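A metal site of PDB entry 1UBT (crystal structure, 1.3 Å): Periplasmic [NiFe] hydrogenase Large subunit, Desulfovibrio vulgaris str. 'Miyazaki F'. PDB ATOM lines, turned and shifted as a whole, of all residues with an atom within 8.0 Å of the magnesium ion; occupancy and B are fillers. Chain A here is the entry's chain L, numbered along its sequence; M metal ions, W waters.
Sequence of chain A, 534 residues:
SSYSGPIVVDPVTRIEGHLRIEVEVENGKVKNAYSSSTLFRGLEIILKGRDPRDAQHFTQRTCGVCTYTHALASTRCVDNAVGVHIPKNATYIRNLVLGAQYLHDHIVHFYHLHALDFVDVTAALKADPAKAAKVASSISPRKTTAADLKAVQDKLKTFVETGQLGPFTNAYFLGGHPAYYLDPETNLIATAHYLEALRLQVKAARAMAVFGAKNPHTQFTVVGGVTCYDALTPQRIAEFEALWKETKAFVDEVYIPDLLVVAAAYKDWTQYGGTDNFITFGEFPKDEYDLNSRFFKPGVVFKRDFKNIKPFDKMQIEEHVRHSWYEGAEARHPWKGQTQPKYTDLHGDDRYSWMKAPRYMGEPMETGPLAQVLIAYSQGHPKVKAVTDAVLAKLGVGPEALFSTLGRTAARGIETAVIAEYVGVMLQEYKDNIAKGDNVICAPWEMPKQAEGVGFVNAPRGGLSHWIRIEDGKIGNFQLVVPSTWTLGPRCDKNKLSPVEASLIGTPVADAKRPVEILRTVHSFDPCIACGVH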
ATOM      1  N   PHE A  40      13.945 -12.079  -2.339  1.00  0.00           N
ATOM      2  CA  PHE A  40      15.345 -11.836  -2.558  1.00  0.00           C
ATOM      3  C   PHE A  40      16.072 -13.208  -2.609  1.00  0.00           C
ATOM      4  O   PHE A  40      15.772 -14.098  -1.784  1.00  0.00           O
ATOM      5  CB  PHE A  40      15.928 -11.031  -1.412  1.00  0.00           C
ATOM      6  CG  PHE A  40      17.414 -10.789  -1.461  1.00  0.00           C
ATOM      7  CD1 PHE A  40      17.960  -9.825  -2.285  1.00  0.00           C
ATOM      8  CD2 PHE A  40      18.278 -11.542  -0.647  1.00  0.00           C
ATOM      9  CE1 PHE A  40      19.327  -9.588  -2.342  1.00  0.00           C
ATOM     10  CE2 PHE A  40      19.652 -11.295  -0.685  1.00  0.00           C
ATOM     11  CZ  PHE A  40      20.192 -10.285  -1.473  1.00  0.00           C
ATOM     12  N   GLU A  44      24.199 -11.830  -6.503  1.00  0.00           N
ATOM     13  CA  GLU A  44      25.458 -11.046  -6.501  1.00  0.00           C
ATOM     14  C   GLU A  44      26.352 -11.403  -5.319  1.00  0.00           C
ATOM     15  O   GLU A  44      27.575 -11.406  -5.429  1.00  0.00           O
ATOM     16  CB  GLU A  44      25.114  -9.556  -6.495  1.00  0.00           C
ATOM     17  CG  GLU A  44      24.449  -9.065  -7.791  1.00  0.00           C
ATOM     18  CD  GLU A  44      23.557  -7.852  -7.557  1.00  0.00           C
ATOM     19  OE1 GLU A  44      23.140  -7.591  -6.407  1.00  0.00           O
ATOM     20  OE2 GLU A  44      23.202  -7.243  -8.583  1.00  0.00           O
ATOM     21  N   GLU A 319      22.365   3.004  -8.503  1.00  0.00           N
ATOM     22  CA  GLU A 319      21.273   2.255  -7.872  1.00  0.00           C
ATOM     23  C   GLU A 319      21.064   2.659  -6.411  1.00  0.00           C
ATOM     24  O   GLU A 319      21.997   2.528  -5.604  1.00  0.00           O
ATOM     25  CB  GLU A 319      21.518   0.744  -7.974  1.00  0.00           C
ATOM     26  CG  GLU A 319      21.578   0.267  -9.428  1.00  0.00           C
ATOM     27  CD  GLU A 319      21.661  -1.265  -9.382  1.00  0.00           C
ATOM     28  OE1 GLU A 319      20.619  -1.919  -9.660  1.00  0.00           O
ATOM     29  OE2 GLU A 319      22.740  -1.780  -9.066  1.00  0.00           O
ATOM     30  N   TYR A 326      17.960  -2.721   1.957  1.00  0.00           N
ATOM     31  CA  TYR A 326      19.409  -2.848   2.002  1.00  0.00           C
ATOM     32  C   TYR A 326      19.961  -1.848   3.009  1.00  0.00           C
ATOM     33  O   TYR A 326      19.272  -0.909   3.407  1.00  0.00           O
ATOM     34  CB  TYR A 326      20.083  -2.625   0.615  1.00  0.00           C
ATOM     35  CG  TYR A 326      19.543  -3.623  -0.388  1.00  0.00           C
ATOM     36  CD1 TYR A 326      18.518  -3.288  -1.269  1.00  0.00           C
ATOM     37  CD2 TYR A 326      20.077  -4.906  -0.409  1.00  0.00           C
ATOM     38  CE1 TYR A 326      18.044  -4.231  -2.180  1.00  0.00           C
ATOM     39  CE2 TYR A 326      19.607  -5.871  -1.300  1.00  0.00           C
ATOM     40  CZ  TYR A 326      18.608  -5.531  -2.172  1.00  0.00           C
ATOM     41  OH  TYR A 326      18.119  -6.491  -3.053  1.00  0.00           O
ATOM     42  N   PRO A 334      27.190   0.684 -10.470  1.00  0.00           N
ATOM     43  CA  PRO A 334      27.371  -0.779 -10.305  1.00  0.00           C
ATOM     44  C   PRO A 334      28.827  -1.243 -10.267  1.00  0.00           C
ATOM     45  O   PRO A 334      29.056  -2.349  -9.719  1.00  0.00           O
ATOM     46  CB  PRO A 334      26.623  -1.410 -11.479  1.00  0.00           C
ATOM     47  CG  PRO A 334      25.939  -0.305 -12.156  1.00  0.00           C
ATOM     48  CD  PRO A 334      26.353   1.028 -11.614  1.00  0.00           C
ATOM     49  N   GLY A 337      29.139  -1.296  -6.743  1.00  0.00           N
ATOM     50  CA  GLY A 337      27.875  -1.706  -6.158  1.00  0.00           C
ATOM     51  C   GLY A 337      28.021  -2.426  -4.828  1.00  0.00           C
ATOM     52  O   GLY A 337      29.081  -2.980  -4.480  1.00  0.00           O
ATOM     53  N   GLN A 338      26.900  -2.421  -4.098  1.00  0.00           N
ATOM     54  CA  GLN A 338      26.828  -3.100  -2.815  1.00  0.00           C
ATOM     55  C   GLN A 338      25.483  -3.813  -2.695  1.00  0.00           C
ATOM     56  O   GLN A 338      24.457  -3.223  -3.115  1.00  0.00           O
ATOM     57  CB  GLN A 338      26.902  -2.142  -1.613  1.00  0.00           C
ATOM     58  CG  GLN A 338      28.204  -1.317  -1.621  1.00  0.00           C
ATOM     59  CD  GLN A 338      28.243  -0.366  -0.425  1.00  0.00           C
ATOM     60  OE1 GLN A 338      29.117  -0.462   0.422  1.00  0.00           O
ATOM     61  NE2 GLN A 338      27.282   0.559  -0.417  1.00  0.00           N
ATOM     62  N   THR A 339      25.534  -5.007  -2.160  1.00  0.00           N
ATOM     63  CA  THR A 339      24.289  -5.787  -1.990  1.00  0.00           C
ATOM     64  C   THR A 339      24.301  -6.331  -0.557  1.00  0.00           C
ATOM     65  O   THR A 339      24.808  -7.418  -0.272  1.00  0.00           O
ATOM     66  CB  THR A 339      24.176  -6.871  -3.061  1.00  0.00           C
ATOM     67  OG1 THR A 339      24.284  -6.207  -4.328  1.00  0.00           O
ATOM     68  CG2 THR A 339      22.826  -7.579  -2.994  1.00  0.00           C
ATOM     69  N   TRP A 354      12.589  -5.392  -2.242  1.00  0.00           N
ATOM     70  CA  TRP A 354      13.916  -5.964  -2.408  1.00  0.00           C
ATOM     71  C   TRP A 354      14.569  -5.460  -3.682  1.00  0.00           C
ATOM     72  O   TRP A 354      15.753  -5.790  -3.886  1.00  0.00           O
ATOM     73  CB  TRP A 354      13.829  -7.508  -2.478  1.00  0.00           C
ATOM     74  CG  TRP A 354      13.586  -8.098  -1.119  1.00  0.00           C
ATOM     75  CD1 TRP A 354      12.453  -8.751  -0.680  1.00  0.00           C
ATOM     76  CD2 TRP A 354      14.489  -8.108   0.016  1.00  0.00           C
ATOM     77  NE1 TRP A 354      12.589  -9.163   0.636  1.00  0.00           N
ATOM     78  CE2 TRP A 354      13.825  -8.785   1.082  1.00  0.00           C
ATOM     79  CE3 TRP A 354      15.792  -7.623   0.195  1.00  0.00           C
ATOM     80  CZ2 TRP A 354      14.450  -8.960   2.333  1.00  0.00           C
ATOM     81  CZ3 TRP A 354      16.400  -7.801   1.433  1.00  0.00           C
ATOM     82  CH2 TRP A 354      15.722  -8.456   2.460  1.00  0.00           C
ATOM     83  N   MET A 355      13.879  -4.723  -4.571  1.00  0.00           N
ATOM     84  CA  MET A 355      14.607  -4.150  -5.681  1.00  0.00           C
ATOM     85  C   MET A 355      15.316  -2.863  -5.265  1.00  0.00           C
ATOM     86  O   MET A 355      14.781  -2.071  -4.476  1.00  0.00           O
ATOM     87  CB  MET A 355      13.660  -3.778  -6.825  1.00  0.00           C
ATOM     88  CG  MET A 355      13.089  -4.988  -7.567  1.00  0.00           C
ATOM     89  SD  MET A 355      12.426  -4.360  -9.153  1.00  0.00           S
ATOM     90  CE  MET A 355      11.291  -5.728  -9.569  1.00  0.00           C
ATOM     91  N   LYS A 356      16.522  -2.675  -5.812  1.00  0.00           N
ATOM     92  CA  LYS A 356      17.165  -1.357  -5.787  1.00  0.00           C
ATOM     93  C   LYS A 356      16.447  -0.440  -6.773  1.00  0.00           C
ATOM     94  O   LYS A 356      15.607  -0.919  -7.565  1.00  0.00           O
ATOM     95  CB  LYS A 356      18.627  -1.461  -6.186  1.00  0.00           C
ATOM     96  CG  LYS A 356      19.445  -2.369  -5.272  1.00  0.00           C
ATOM     97  CD  LYS A 356      20.877  -2.538  -5.790  1.00  0.00           C
ATOM     98  CE  LYS A 356      21.727  -3.383  -4.825  1.00  0.00           C
ATOM     99  NZ  LYS A 356      23.020  -3.771  -5.487  1.00  0.00           N
ATOM    100  N   PRO A 358      17.273   1.968  -9.684  1.00  0.00           N
ATOM    101  CA  PRO A 358      18.226   2.589 -10.615  1.00  0.00           C
ATOM    102  C   PRO A 358      17.728   3.946 -11.082  1.00  0.00           C
ATOM    103  O   PRO A 358      16.558   4.113 -11.400  1.00  0.00           O
ATOM    104  CB  PRO A 358      18.288   1.593 -11.773  1.00  0.00           C
ATOM    105  CG  PRO A 358      17.702   0.316 -11.244  1.00  0.00           C
ATOM    106  CD  PRO A 358      16.626   0.807 -10.276  1.00  0.00           C
ATOM    107  N   SER A 465      22.265  -4.849 -17.847  1.00  0.00           N
ATOM    108  CA  SER A 465      23.724  -4.702 -17.839  1.00  0.00           C
ATOM    109  C   SER A 465      24.282  -5.541 -16.671  1.00  0.00           C
ATOM    110  O   SER A 465      23.704  -5.596 -15.577  1.00  0.00           O
ATOM    111  CB  SER A 465      24.136  -3.224 -17.753  1.00  0.00           C
ATOM    112  OG  SER A 465      23.527  -2.510 -16.693  1.00  0.00           O
ATOM    113  N   TRP A 467      27.985  -6.169 -14.617  1.00  0.00           N
ATOM    114  CA  TRP A 467      29.189  -5.376 -14.353  1.00  0.00           C
ATOM    115  C   TRP A 467      30.134  -6.191 -13.480  1.00  0.00           C
ATOM    116  O   TRP A 467      29.681  -6.656 -12.429  1.00  0.00           O
ATOM    117  CB  TRP A 467      28.784  -4.119 -13.603  1.00  0.00           C
ATOM    118  CG  TRP A 467      27.740  -3.277 -14.269  1.00  0.00           C
ATOM    119  CD1 TRP A 467      26.408  -3.478 -14.375  1.00  0.00           C
ATOM    120  CD2 TRP A 467      28.020  -2.016 -14.958  1.00  0.00           C
ATOM    121  NE1 TRP A 467      25.830  -2.420 -15.072  1.00  0.00           N
ATOM    122  CE2 TRP A 467      26.796  -1.523 -15.437  1.00  0.00           C
ATOM    123  CE3 TRP A 467      29.193  -1.286 -15.182  1.00  0.00           C
ATOM    124  CZ2 TRP A 467      26.721  -0.314 -16.150  1.00  0.00           C
ATOM    125  CZ3 TRP A 467      29.114  -0.099 -15.893  1.00  0.00           C
ATOM    126  CH2 TRP A 467      27.896   0.385 -16.364  1.00  0.00           C
ATOM    127  N   PHE A 478      30.311  -8.355  -8.587  1.00  0.00           N
ATOM    128  CA  PHE A 478      29.540  -8.656  -9.813  1.00  0.00           C
ATOM    129  C   PHE A 478      28.172  -8.024  -9.536  1.00  0.00           C
ATOM    130  O   PHE A 478      27.540  -8.398  -8.540  1.00  0.00           O
ATOM    131  CB  PHE A 478      29.431 -10.151 -10.084  1.00  0.00           C
ATOM    132  CG  PHE A 478      29.082 -10.448 -11.545  1.00  0.00           C
ATOM    133  CD1 PHE A 478      27.778 -10.204 -11.975  1.00  0.00           C
ATOM    134  CD2 PHE A 478      30.011 -10.916 -12.451  1.00  0.00           C
ATOM    135  CE1 PHE A 478      27.472 -10.456 -13.300  1.00  0.00           C
ATOM    136  CE2 PHE A 478      29.690 -11.160 -13.780  1.00  0.00           C
ATOM    137  CZ  PHE A 478      28.397 -10.902 -14.226  1.00  0.00           C
ATOM    138  N   GLN A 479      27.756  -7.117 -10.405  1.00  0.00           N
ATOM    139  CA  GLN A 479      26.456  -6.437 -10.151  1.00  0.00           C
ATOM    140  C   GLN A 479      25.572  -6.597 -11.387  1.00  0.00           C
ATOM    141  O   GLN A 479      26.058  -6.323 -12.501  1.00  0.00           O
ATOM    142  CB  GLN A 479      26.687  -4.963  -9.829  1.00  0.00           C
ATOM    143  CG  GLN A 479      27.403  -4.730  -8.475  1.00  0.00           C
ATOM    144  CD  GLN A 479      26.529  -5.115  -7.301  1.00  0.00           C
ATOM    145  OE1 GLN A 479      25.317  -4.878  -7.319  1.00  0.00           O
ATOM    146  NE2 GLN A 479      27.151  -5.648  -6.253  1.00  0.00           N
ATOM    147  N   LEU A 480      24.314  -6.994 -11.174  1.00  0.00           N
ATOM    148  CA  LEU A 480      23.321  -6.993 -12.219  1.00  0.00           C
ATOM    149  C   LEU A 480      22.404  -5.787 -12.063  1.00  0.00           C
ATOM    150  O   LEU A 480      21.984  -5.530 -10.967  1.00  0.00           O
ATOM    151  CB  LEU A 480      22.437  -8.256 -12.190  1.00  0.00           C
ATOM    152  CG  LEU A 480      23.130  -9.625 -12.146  1.00  0.00           C
ATOM    153  CD1 LEU A 480      22.057 -10.616 -12.601  1.00  0.00           C
ATOM    154  CD2 LEU A 480      24.306  -9.667 -12.993  1.00  0.00           C
ATOM    155  N   VAL A 481      22.141  -5.070 -13.145  1.00  0.00           N
ATOM    156  CA  VAL A 481      21.182  -3.960 -13.125  1.00  0.00           C
ATOM    157  C   VAL A 481      20.212  -4.367 -14.253  1.00  0.00           C
ATOM    158  O   VAL A 481      20.613  -4.424 -15.416  1.00  0.00           O
ATOM    159  CB  VAL A 481      21.775  -2.584 -13.422  1.00  0.00           C
ATOM    160  CG1 VAL A 481      20.703  -1.486 -13.244  1.00  0.00           C
ATOM    161  CG2 VAL A 481      22.987  -2.334 -12.539  1.00  0.00           C
ATOM    162  N   VAL A 482      18.978  -4.713 -13.895  1.00  0.00           N
ATOM    163  CA  VAL A 482      18.145  -5.474 -14.826  1.00  0.00           C
ATOM    164  C   VAL A 482      16.975  -4.632 -15.284  1.00  0.00           C
ATOM    165  O   VAL A 482      16.574  -3.692 -14.538  1.00  0.00           O
ATOM    166  CB  VAL A 482      17.751  -6.756 -14.079  1.00  0.00           C
ATOM    167  CG1 VAL A 482      16.989  -7.723 -14.958  1.00  0.00           C
ATOM    168  CG2 VAL A 482      19.010  -7.480 -13.587  1.00  0.00           C
ATOM    169  N   THR A 485      14.369  -3.893 -12.797  1.00  0.00           N
ATOM    170  CA  THR A 485      14.829  -3.067 -11.701  1.00  0.00           C
ATOM    171  C   THR A 485      14.563  -1.586 -12.002  1.00  0.00           C
ATOM    172  O   THR A 485      14.048  -0.847 -11.157  1.00  0.00           O
ATOM    173  CB  THR A 485      16.347  -3.273 -11.468  1.00  0.00           C
ATOM    174  OG1 THR A 485      16.730  -4.656 -11.615  1.00  0.00           O
ATOM    175  CG2 THR A 485      16.712  -2.811 -10.069  1.00  0.00           C
ATOM    176  N   CYS A 531      14.190 -11.280 -12.086  1.00  0.00           N
ATOM    177  CA  CYS A 531      15.084 -10.370 -12.773  1.00  0.00           C
ATOM    178  C   CYS A 531      15.365  -9.120 -11.942  1.00  0.00           C
ATOM    179  O   CYS A 531      16.500  -8.726 -11.735  1.00  0.00           O
ATOM    180  CB  CYS A 531      14.486  -9.911 -14.114  1.00  0.00           C
ATOM    181  SG  CYS A 531      15.063 -11.000 -15.463  1.00  0.00           S
ATOM    182  N   GLY A 532      14.306  -8.443 -11.483  1.00  0.00           N
ATOM    183  CA  GLY A 532      14.563  -7.128 -10.897  1.00  0.00           C
ATOM    184  C   GLY A 532      15.369  -7.184  -9.634  1.00  0.00           C
ATOM    185  O   GLY A 532      16.147  -6.275  -9.379  1.00  0.00           O
ATOM    186  N   VAL A 533      15.178  -8.223  -8.831  1.00  0.00           N
ATOM    187  CA  VAL A 533      15.855  -8.363  -7.527  1.00  0.00           C
ATOM    188  C   VAL A 533      17.096  -9.228  -7.541  1.00  0.00           C
ATOM    189  O   VAL A 533      18.128  -8.890  -6.948  1.00  0.00           O
ATOM    190  CB  VAL A 533      14.938  -9.011  -6.469  1.00  0.00           C
ATOM    191  CG1 VAL A 533      15.661  -9.195  -5.144  1.00  0.00           C
ATOM    192  CG2 VAL A 533      13.662  -8.207  -6.259  1.00  0.00           C
ATOM    193  N   HIS A 534      17.085 -10.384  -8.239  1.00  0.00           N
ATOM    194  CA  HIS A 534      18.206 -11.330  -8.305  1.00  0.00           C
ATOM    195  C   HIS A 534      18.809 -11.581  -6.887  1.00  0.00           C
ATOM    196  O   HIS A 534      17.879 -11.797  -5.942  1.00  0.00           O
ATOM    197  CB  HIS A 534      19.290 -10.970  -9.326  1.00  0.00           C
ATOM    198  CG  HIS A 534      19.652  -9.529  -9.451  1.00  0.00           C
ATOM    199  ND1 HIS A 534      18.794  -8.639 -10.110  1.00  0.00           N
ATOM    200  CD2 HIS A 534      20.639  -8.784  -8.911  1.00  0.00           C
ATOM    201  CE1 HIS A 534      19.326  -7.426  -9.997  1.00  0.00           C
ATOM    202  NE2 HIS A 534      20.434  -7.497  -9.289  1.00  0.00           N
ATOM    203  OXT HIS A 534      19.960 -11.648  -6.670  1.00  0.00           O
HETATM  204 MG    MG M   1      21.666  -5.790  -8.863  1.00  0.00          MG
HETATM  205  O   HOH W   1      20.134  -4.411  -8.946  1.00  0.00           O
HETATM  206  O   HOH W   2      21.168  -5.823  -6.836  1.00  0.00           O
HETATM  207  O   HOH W   3      22.946  -4.197  -8.519  1.00  0.00           O
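Water W2 lies within hydrogen-bond range of the side-chain carboxylate of Glu 44 (2.7 Å) and the side-chain amino group of Lys 356 (3.1 Å).
Water W3 lies within hydrogen-bond range of OE2 of Glu 319, OE1 of Gln 479 and NZ of Lys 356.
OE1 of Glu 44 lies within salt-bridge range of NZ of Lys 356 (3.9 Å).
The backbone carbonyl oxygen of Cys 531 is in hydrogen-bond range of a ring nitrogen (ND1) of His 534 (2.8 Å).
The side-chain hydroxyl (OG1) of Thr 339 sits at hydrogen-bond distance from the side-chain carboxylate (OE1) of Glu 44.
The side-chain carboxylate of Glu 44 sits close to the side-chain amide oxygen of Gln 479, 3.4 Å away.
Of the 24 residues printed, 3 come within 4 Å of the magnesium ion.
The nearest printed residue that does not touch the magnesium ion is Gln 479 (4.1 Å).
The magnesium ion is bound by water W1 (2.1 Å), water W3 (2.1 Å), water W2 (2.1 Å), the side-chain carboxylate (OE2) of Glu 44 (2.1 Å), the backbone carbonyl oxygen (O) of Leu 480 (2.1 Å) and a ring nitrogen (NE2) of His 534 (2.1 Å).
The magnesium ion has six donor atoms within binding distance.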
